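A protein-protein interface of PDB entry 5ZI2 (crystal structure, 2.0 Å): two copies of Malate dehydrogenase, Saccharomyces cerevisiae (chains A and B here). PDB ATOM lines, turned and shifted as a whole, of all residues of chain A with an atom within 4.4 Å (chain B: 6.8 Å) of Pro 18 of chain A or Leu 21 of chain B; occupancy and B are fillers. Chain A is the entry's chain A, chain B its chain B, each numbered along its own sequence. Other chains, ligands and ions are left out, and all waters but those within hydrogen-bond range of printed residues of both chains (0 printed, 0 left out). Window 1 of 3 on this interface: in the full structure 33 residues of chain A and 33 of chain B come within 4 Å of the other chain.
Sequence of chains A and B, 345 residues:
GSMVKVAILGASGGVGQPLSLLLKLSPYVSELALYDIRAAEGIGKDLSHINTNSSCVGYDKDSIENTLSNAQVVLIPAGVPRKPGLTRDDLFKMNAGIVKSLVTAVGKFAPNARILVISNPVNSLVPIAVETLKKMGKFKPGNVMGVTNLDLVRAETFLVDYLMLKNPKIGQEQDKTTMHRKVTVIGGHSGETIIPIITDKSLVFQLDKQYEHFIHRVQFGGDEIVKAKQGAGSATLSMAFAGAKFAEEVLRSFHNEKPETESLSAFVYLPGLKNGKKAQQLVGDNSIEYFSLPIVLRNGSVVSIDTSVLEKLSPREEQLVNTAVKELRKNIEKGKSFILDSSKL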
ATOM      1  N   GLY A  13     -30.191  -4.129  10.093  1.00  0.00           N
ATOM      2  CA  GLY A  13     -30.975  -3.082  10.690  1.00  0.00           C
ATOM      3  C   GLY A  13     -30.749  -1.712  10.114  1.00  0.00           C
ATOM      4  O   GLY A  13     -29.962  -1.528   9.140  1.00  0.00           O
ATOM      5  N   GLY A  14     -31.396  -0.781  10.791  1.00  0.00           N
ATOM      6  CA  GLY A  14     -31.312   0.654  10.530  1.00  0.00           C
ATOM      7  C   GLY A  14     -29.889   1.212  10.498  1.00  0.00           C
ATOM      8  O   GLY A  14     -29.499   1.874   9.560  1.00  0.00           O
ATOM      9  N   VAL A  15     -29.132   0.873  11.513  1.00  0.00           N
ATOM     10  CA  VAL A  15     -27.736   1.248  11.620  1.00  0.00           C
ATOM     11  C   VAL A  15     -26.929   0.250  10.806  1.00  0.00           C
ATOM     12  O   VAL A  15     -26.053   0.631  10.066  1.00  0.00           O
ATOM     13  CB  VAL A  15     -27.275   1.237  13.077  1.00  0.00           C
ATOM     14  CG1 VAL A  15     -25.754   1.438  13.200  1.00  0.00           C
ATOM     15  CG2 VAL A  15     -28.052   2.295  13.914  1.00  0.00           C
ATOM     16  N   GLY A  16     -27.214  -1.045  10.984  1.00  0.00           N
ATOM     17  CA  GLY A  16     -26.447  -2.141  10.402  1.00  0.00           C
ATOM     18  C   GLY A  16     -26.255  -2.070   8.896  1.00  0.00           C
ATOM     19  O   GLY A  16     -25.161  -2.333   8.367  1.00  0.00           O
ATOM     20  N   GLN A  17     -27.300  -1.734   8.184  1.00  0.00           N
ATOM     21  CA  GLN A  17     -27.163  -1.720   6.735  1.00  0.00           C
ATOM     22  C   GLN A  17     -26.198  -0.671   6.193  1.00  0.00           C
ATOM     23  O   GLN A  17     -25.306  -1.011   5.436  1.00  0.00           O
ATOM     24  CB  GLN A  17     -28.520  -1.554   6.053  1.00  0.00           C
ATOM     25  CG  GLN A  17     -29.282  -2.842   5.942  1.00  0.00           C
ATOM     26  CD  GLN A  17     -30.424  -2.752   4.961  1.00  0.00           C
ATOM     27  OE1 GLN A  17     -30.231  -2.386   3.820  1.00  0.00           O
ATOM     28  NE2 GLN A  17     -31.584  -3.204   5.383  1.00  0.00           N
ATOM     29  N   PRO A  18     -26.427   0.600   6.499  1.00  0.00           N
ATOM     30  CA  PRO A  18     -25.460   1.614   6.050  1.00  0.00           C
ATOM     31  C   PRO A  18     -24.070   1.457   6.700  1.00  0.00           C
ATOM     32  O   PRO A  18     -23.050   1.814   6.084  1.00  0.00           O
ATOM     33  CB  PRO A  18     -26.143   2.947   6.418  1.00  0.00           C
ATOM     34  CG  PRO A  18     -27.091   2.635   7.496  1.00  0.00           C
ATOM     35  CD  PRO A  18     -27.594   1.231   7.126  1.00  0.00           C
ATOM     36  N   LEU A  19     -24.027   0.920   7.925  1.00  0.00           N
ATOM     37  CA  LEU A  19     -22.757   0.589   8.539  1.00  0.00           C
ATOM     38  C   LEU A  19     -22.023  -0.454   7.710  1.00  0.00           C
ATOM     39  O   LEU A  19     -20.792  -0.293   7.425  1.00  0.00           O
ATOM     40  CB  LEU A  19     -22.900   0.119   9.991  1.00  0.00           C
ATOM     41  CG  LEU A  19     -21.664  -0.331  10.738  1.00  0.00           C
ATOM     42  CD1 LEU A  19     -20.786   0.868  11.073  1.00  0.00           C
ATOM     43  CD2 LEU A  19     -22.069  -1.087  12.017  1.00  0.00           C
ATOM     44  N   SER A  20     -22.751  -1.485   7.269  1.00  0.00           N
ATOM     45  CA  SER A  20     -22.171  -2.483   6.404  1.00  0.00           C
ATOM     46  C   SER A  20     -21.679  -1.909   5.069  1.00  0.00           C
ATOM     47  O   SER A  20     -20.620  -2.278   4.615  1.00  0.00           O
ATOM     48  CB  SER A  20     -23.126  -3.666   6.162  1.00  0.00           C
ATOM     49  OG  SER A  20     -23.546  -4.223   7.433  1.00  0.00           O
ATOM     50  N   LEU A  21     -22.482  -1.031   4.459  1.00  0.00           N
ATOM     51  CA  LEU A  21     -22.066  -0.323   3.249  1.00  0.00           C
ATOM     52  C   LEU A  21     -20.749   0.448   3.478  1.00  0.00           C
ATOM     53  O   LEU A  21     -19.797   0.293   2.706  1.00  0.00           O
ATOM     54  CB  LEU A  21     -23.137   0.658   2.778  1.00  0.00           C
ATOM     55  CG  LEU A  21     -22.728   1.635   1.650  1.00  0.00           C
ATOM     56  CD1 LEU A  21     -22.320   0.905   0.369  1.00  0.00           C
ATOM     57  CD2 LEU A  21     -23.882   2.589   1.404  1.00  0.00           C
ATOM     58  N   LEU A  22     -20.695   1.281   4.510  1.00  0.00           N
ATOM     59  CA  LEU A  22     -19.442   2.017   4.754  1.00  0.00           C
ATOM     60  C   LEU A  22     -18.266   1.085   5.044  1.00  0.00           C
ATOM     61  O   LEU A  22     -17.183   1.319   4.574  1.00  0.00           O
ATOM     62  CB  LEU A  22     -19.611   3.030   5.860  1.00  0.00           C
ATOM     63  CG  LEU A  22     -20.653   4.110   5.507  1.00  0.00           C
ATOM     64  CD1 LEU A  22     -20.874   5.011   6.710  1.00  0.00           C
ATOM     65  CD2 LEU A  22     -20.154   4.926   4.306  1.00  0.00           C
ATOM     66  N   LEU A 237     -28.385   6.799  10.097  1.00  0.00           N
ATOM     67  CA  LEU A 237     -27.346   7.052   9.085  1.00  0.00           C
ATOM     68  C   LEU A 237     -26.119   7.728   9.740  1.00  0.00           C
ATOM     69  O   LEU A 237     -24.946   7.414   9.430  1.00  0.00           O
ATOM     70  CB  LEU A 237     -27.925   7.926   7.947  1.00  0.00           C
ATOM     71  CG  LEU A 237     -29.133   7.334   7.192  1.00  0.00           C
ATOM     72  CD1 LEU A 237     -29.790   8.327   6.276  1.00  0.00           C
ATOM     73  CD2 LEU A 237     -28.723   6.118   6.367  1.00  0.00           C
ATOM     74  N   ALA A 240     -24.345   5.054  11.758  1.00  0.00           N
ATOM     75  CA  ALA A 240     -23.541   4.238  10.829  1.00  0.00           C
ATOM     76  C   ALA A 240     -22.208   4.993  10.434  1.00  0.00           C
ATOM     77  O   ALA A 240     -21.107   4.418  10.433  1.00  0.00           O
ATOM     78  CB  ALA A 240     -24.350   3.927   9.620  1.00  0.00           C
ATOM     79  N   ILE B   8     -31.875  15.691  -3.771  1.00  0.00           N
ATOM     80  CA  ILE B   8     -32.239  14.316  -3.971  1.00  0.00           C
ATOM     81  C   ILE B   8     -33.745  14.195  -3.841  1.00  0.00           C
ATOM     82  O   ILE B   8     -34.328  14.494  -2.780  1.00  0.00           O
ATOM     83  CB  ILE B   8     -31.566  13.392  -2.956  1.00  0.00           C
ATOM     84  CG1 ILE B   8     -30.041  13.532  -3.146  1.00  0.00           C
ATOM     85  CG2 ILE B   8     -31.934  11.899  -3.233  1.00  0.00           C
ATOM     86  CD1 ILE B   8     -29.236  12.568  -2.375  1.00  0.00           C
ATOM     87  N   GLY B  16     -32.516   5.744  -1.925  1.00  0.00           N
ATOM     88  CA  GLY B  16     -32.348   7.153  -1.543  1.00  0.00           C
ATOM     89  C   GLY B  16     -31.657   7.405  -0.219  1.00  0.00           C
ATOM     90  O   GLY B  16     -30.890   8.384  -0.096  1.00  0.00           O
ATOM     91  N   GLN B  17     -31.933   6.581   0.802  1.00  0.00           N
ATOM     92  CA  GLN B  17     -31.266   6.837   2.108  1.00  0.00           C
ATOM     93  C   GLN B  17     -29.765   6.670   2.057  1.00  0.00           C
ATOM     94  O   GLN B  17     -29.053   7.561   2.478  1.00  0.00           O
ATOM     95  CB  GLN B  17     -31.848   6.026   3.263  1.00  0.00           C
ATOM     96  CG  GLN B  17     -33.254   6.420   3.601  1.00  0.00           C
ATOM     97  CD  GLN B  17     -33.634   5.990   4.999  1.00  0.00           C
ATOM     98  OE1 GLN B  17     -32.782   5.910   5.913  1.00  0.00           O
ATOM     99  NE2 GLN B  17     -34.927   5.783   5.205  1.00  0.00           N
ATOM    100  N   PRO B  18     -29.283   5.534   1.587  1.00  0.00           N
ATOM    101  CA  PRO B  18     -27.850   5.381   1.524  1.00  0.00           C
ATOM    102  C   PRO B  18     -27.158   6.294   0.510  1.00  0.00           C
ATOM    103  O   PRO B  18     -26.002   6.739   0.746  1.00  0.00           O
ATOM    104  CB  PRO B  18     -27.680   3.877   1.175  1.00  0.00           C
ATOM    105  CG  PRO B  18     -28.944   3.488   0.492  1.00  0.00           C
ATOM    106  CD  PRO B  18     -29.968   4.242   1.313  1.00  0.00           C
ATOM    107  N   LEU B  19     -27.869   6.615  -0.552  1.00  0.00           N
ATOM    108  CA  LEU B  19     -27.465   7.648  -1.499  1.00  0.00           C
ATOM    109  C   LEU B  19     -27.265   9.015  -0.836  1.00  0.00           C
ATOM    110  O   LEU B  19     -26.169   9.626  -0.921  1.00  0.00           O
ATOM    111  CB  LEU B  19     -28.475   7.779  -2.632  1.00  0.00           C
ATOM    112  CG  LEU B  19     -28.076   8.744  -3.728  1.00  0.00           C
ATOM    113  CD1 LEU B  19     -26.878   8.213  -4.486  1.00  0.00           C
ATOM    114  CD2 LEU B  19     -29.218   9.035  -4.670  1.00  0.00           C
ATOM    115  N   SER B  20     -28.275   9.420  -0.058  1.00  0.00           N
ATOM    116  CA  SER B  20     -28.173  10.689   0.701  1.00  0.00           C
ATOM    117  C   SER B  20     -26.973  10.665   1.669  1.00  0.00           C
ATOM    118  O   SER B  20     -26.254  11.656   1.768  1.00  0.00           O
ATOM    119  CB  SER B  20     -29.476  10.976   1.387  1.00  0.00           C
ATOM    120  OG  SER B  20     -30.537  10.931   0.482  1.00  0.00           O
ATOM    121  N   LEU B  21     -26.759   9.526   2.379  1.00  0.00           N
ATOM    122  CA  LEU B  21     -25.580   9.376   3.225  1.00  0.00           C
ATOM    123  C   LEU B  21     -24.249   9.580   2.444  1.00  0.00           C
ATOM    124  O   LEU B  21     -23.375  10.366   2.852  1.00  0.00           O
ATOM    125  CB  LEU B  21     -25.599   7.975   3.865  1.00  0.00           C
ATOM    126  CG  LEU B  21     -24.323   7.576   4.573  1.00  0.00           C
ATOM    127  CD1 LEU B  21     -23.990   8.569   5.703  1.00  0.00           C
ATOM    128  CD2 LEU B  21     -24.541   6.227   5.188  1.00  0.00           C
ATOM    129  N   LEU B  22     -24.067   8.828   1.373  1.00  0.00           N
ATOM    130  CA  LEU B  22     -22.847   8.998   0.572  1.00  0.00           C
ATOM    131  C   LEU B  22     -22.660  10.441   0.021  1.00  0.00           C
ATOM    132  O   LEU B  22     -21.550  11.007   0.109  1.00  0.00           O
ATOM    133  CB  LEU B  22     -22.802   7.991  -0.540  1.00  0.00           C
ATOM    134  CG  LEU B  22     -22.693   6.542  -0.054  1.00  0.00           C
ATOM    135  CD1 LEU B  22     -22.729   5.599  -1.234  1.00  0.00           C
ATOM    136  CD2 LEU B  22     -21.429   6.328   0.761  1.00  0.00           C
ATOM    137  N   LEU B  23     -23.767  11.076  -0.378  1.00  0.00           N
ATOM    138  CA  LEU B  23     -23.724  12.484  -0.795  1.00  0.00           C
ATOM    139  C   LEU B  23     -23.328  13.429   0.306  1.00  0.00           C
ATOM    140  O   LEU B  23     -22.502  14.321   0.081  1.00  0.00           O
ATOM    141  CB  LEU B  23     -24.956  12.949  -1.543  1.00  0.00           C
ATOM    142  CG  LEU B  23     -24.981  12.889  -3.062  1.00  0.00           C
ATOM    143  CD1 LEU B  23     -23.946  13.764  -3.691  1.00  0.00           C
ATOM    144  CD2 LEU B  23     -24.728  11.482  -3.476  1.00  0.00           C
ATOM    145  N   LYS B  24     -23.850  13.192   1.493  1.00  0.00           N
ATOM    146  CA  LYS B  24     -23.433  13.991   2.647  1.00  0.00           C
ATOM    147  C   LYS B  24     -21.943  13.953   2.911  1.00  0.00           C
ATOM    148  O   LYS B  24     -21.420  14.935   3.332  1.00  0.00           O
ATOM    149  CB  LYS B  24     -24.179  13.580   3.920  1.00  0.00           C
ATOM    150  CG  LYS B  24     -23.865  14.415   5.161  1.00  0.00           C
ATOM    151  CD  LYS B  24     -24.363  15.827   5.058  1.00  0.00           C
ATOM    152  CE  LYS B  24     -24.102  16.715   6.271  1.00  0.00           C
ATOM    153  NZ  LYS B  24     -22.835  17.541   6.182  1.00  0.00           N
ATOM    154  N   LEU B  25     -21.304  12.813   2.677  1.00  0.00           N
ATOM    155  CA  LEU B  25     -19.863  12.665   2.854  1.00  0.00           C
ATOM    156  C   LEU B  25     -19.014  13.304   1.767  1.00  0.00           C
ATOM    157  O   LEU B  25     -17.825  13.362   1.940  1.00  0.00           O
ATOM    158  CB  LEU B  25     -19.463  11.203   2.876  1.00  0.00           C
ATOM    159  CG  LEU B  25     -20.294  10.370   3.810  1.00  0.00           C
ATOM    160  CD1 LEU B  25     -19.667   9.026   4.001  1.00  0.00           C
ATOM    161  CD2 LEU B  25     -20.490  11.054   5.155  1.00  0.00           C
ATOM    162  N   SER B  26     -19.597  13.728   0.635  1.00  0.00           N
ATOM    163  CA  SER B  26     -18.787  14.316  -0.441  1.00  0.00           C
ATOM    164  C   SER B  26     -18.220  15.718  -0.100  1.00  0.00           C
ATOM    165  O   SER B  26     -18.939  16.652   0.255  1.00  0.00           O
ATOM    166  CB  SER B  26     -19.586  14.436  -1.692  1.00  0.00           C
ATOM    167  OG  SER B  26     -18.801  15.070  -2.724  1.00  0.00           O
ATOM    168  N   LEU B  32     -27.100  20.066   0.583  1.00  0.00           N
ATOM    169  CA  LEU B  32     -27.774  18.892   0.160  1.00  0.00           C
ATOM    170  C   LEU B  32     -29.210  19.023   0.623  1.00  0.00           C
ATOM    171  O   LEU B  32     -29.442  19.156   1.822  1.00  0.00           O
ATOM    172  CB  LEU B  32     -27.087  17.731   0.855  1.00  0.00           C
ATOM    173  CG  LEU B  32     -27.655  16.336   0.556  1.00  0.00           C
ATOM    174  CD1 LEU B  32     -27.757  16.058  -0.915  1.00  0.00           C
ATOM    175  CD2 LEU B  32     -26.841  15.305   1.292  1.00  0.00           C
ATOM    176  N   LEU B  34     -32.993  17.254   0.582  1.00  0.00           N
ATOM    177  CA  LEU B  34     -33.590  15.980   0.437  1.00  0.00           C
ATOM    178  C   LEU B  34     -35.086  16.168   0.417  1.00  0.00           C
ATOM    179  O   LEU B  34     -35.625  16.947   1.203  1.00  0.00           O
ATOM    180  CB  LEU B  34     -33.237  15.106   1.644  1.00  0.00           C
ATOM    181  CG  LEU B  34     -31.744  14.965   2.001  1.00  0.00           C
ATOM    182  CD1 LEU B  34     -31.635  13.949   3.153  1.00  0.00           C
ATOM    183  CD2 LEU B  34     -30.964  14.486   0.752  1.00  0.00           C
ATOM    184  N   ILE B  43     -34.723  12.332   7.953  1.00  0.00           N
ATOM    185  CA  ILE B  43     -33.498  11.814   7.347  1.00  0.00           C
ATOM    186  C   ILE B  43     -32.482  12.918   7.206  1.00  0.00           C
ATOM    187  O   ILE B  43     -31.320  12.705   7.474  1.00  0.00           O
ATOM    188  CB  ILE B  43     -33.783  11.143   5.989  1.00  0.00           C
ATOM    189  CG1 ILE B  43     -34.553   9.871   6.282  1.00  0.00           C
ATOM    190  CG2 ILE B  43     -32.501  10.802   5.189  1.00  0.00           C
ATOM    191  CD1 ILE B  43     -35.353   9.498   5.108  1.00  0.00           C
ATOM    192  N   LEU B  47     -28.811  13.119   8.931  1.00  0.00           N
ATOM    193  CA  LEU B  47     -27.575  13.437   8.177  1.00  0.00           C
ATOM    194  C   LEU B  47     -26.886  14.738   8.581  1.00  0.00           C
ATOM    195  O   LEU B  47     -25.646  14.871   8.497  1.00  0.00           O
ATOM    196  CB  LEU B  47     -27.893  13.401   6.699  1.00  0.00           C
ATOM    197  CG  LEU B  47     -28.215  11.967   6.217  1.00  0.00           C
ATOM    198  CD1 LEU B  47     -28.683  12.047   4.782  1.00  0.00           C
ATOM    199  CD2 LEU B  47     -26.976  11.063   6.361  1.00  0.00           C
ATOM    200  N   ILE B  50     -23.729  14.814  10.781  1.00  0.00           N
ATOM    201  CA  ILE B  50     -22.467  14.320  10.286  1.00  0.00           C
ATOM    202  C   ILE B  50     -21.482  15.483  10.067  1.00  0.00           C
ATOM    203  O   ILE B  50     -21.864  16.509   9.511  1.00  0.00           O
ATOM    204  CB  ILE B  50     -22.650  13.450   9.036  1.00  0.00           C
ATOM    205  CG1 ILE B  50     -23.381  12.142   9.399  1.00  0.00           C
ATOM    206  CG2 ILE B  50     -21.322  13.110   8.409  1.00  0.00           C
ATOM    207  CD1 ILE B  50     -23.780  11.296   8.252  1.00  0.00           C
ATOM    208  N   LEU B 237     -28.085  -0.912  -1.865  1.00  0.00           N
ATOM    209  CA  LEU B 237     -26.827  -0.383  -1.334  1.00  0.00           C
ATOM    210  C   LEU B 237     -25.779  -0.208  -2.425  1.00  0.00           C
ATOM    211  O   LEU B 237     -25.178   0.819  -2.481  1.00  0.00           O
ATOM    212  CB  LEU B 237     -26.269  -1.307  -0.256  1.00  0.00           C
ATOM    213  CG  LEU B 237     -27.178  -1.461   0.985  1.00  0.00           C
ATOM    214  CD1 LEU B 237     -26.615  -2.469   1.981  1.00  0.00           C
ATOM    215  CD2 LEU B 237     -27.367  -0.106   1.678  1.00  0.00           C
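Leu 237 of chain B touches Gln 17 of chain A (CD1 to O, 3.97 Å).
Leu 21 of chain B touches Pro 18 of chain A (CD2 to CB, 3.9 Å).
Leu 237 of chain A touches Gln 17 of chain B.
Ile 43 of chain B touches Leu 237 of chain A (CG2 to CD1, 3.8 Å).
CB of Leu 237 of chain A touches CD2 of Leu 47 of chain B, 3.6 Å away.
Printed residues of chain B within 4 Å of Gln 17 of chain A: Leu 237 (3.97 Å).
Of the printed residues of chain B, Pro 18 of chain A touches Leu 21 (3.9 Å).
Printed residues of chain A within 4 Å of Gln 17 of chain B: Leu 237 (3.9 Å).
Of the printed residues of chain A, Leu 21 of chain B touches Pro 18 (3.9 Å).
Ile 50 of chain B touches none of the printed residues of chain A.
Of the printed residues of chain A, Leu 237 of chain B touches Gln 17.
Printed residues of chain B that touch a printed residue of chain A: Gln 17, Leu 21, Ile 43, Leu 47 and Leu 237.
Hydrophobic or aromatic side chains of chain B that line the printed part of chain A: Leu 21, Ile 43, Leu 47 and Leu 237.
Of the 12 printed residues of chain A, 3 touch a printed residue of chain B.
Printed residues of chain A that touch a printed residue of chain B: Gln 17, Pro 18 and Leu 237.
Hydrophobic or aromatic side chains of chain A that line the printed part of chain B: Pro 18 and Leu 237.
Among the printed residues, 5 pairs touch across the chains.
Gln 17 of chain A touches Leu 237 of chain B, and with the chains exchanged Leu 237 of chain A touches Gln 17 of chain B.
Pro 18 of chain A touches Leu 21 of chain B, but with the chains exchanged Leu 21 of chain A does not touch Pro 18 of chain B (4.02 Å).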
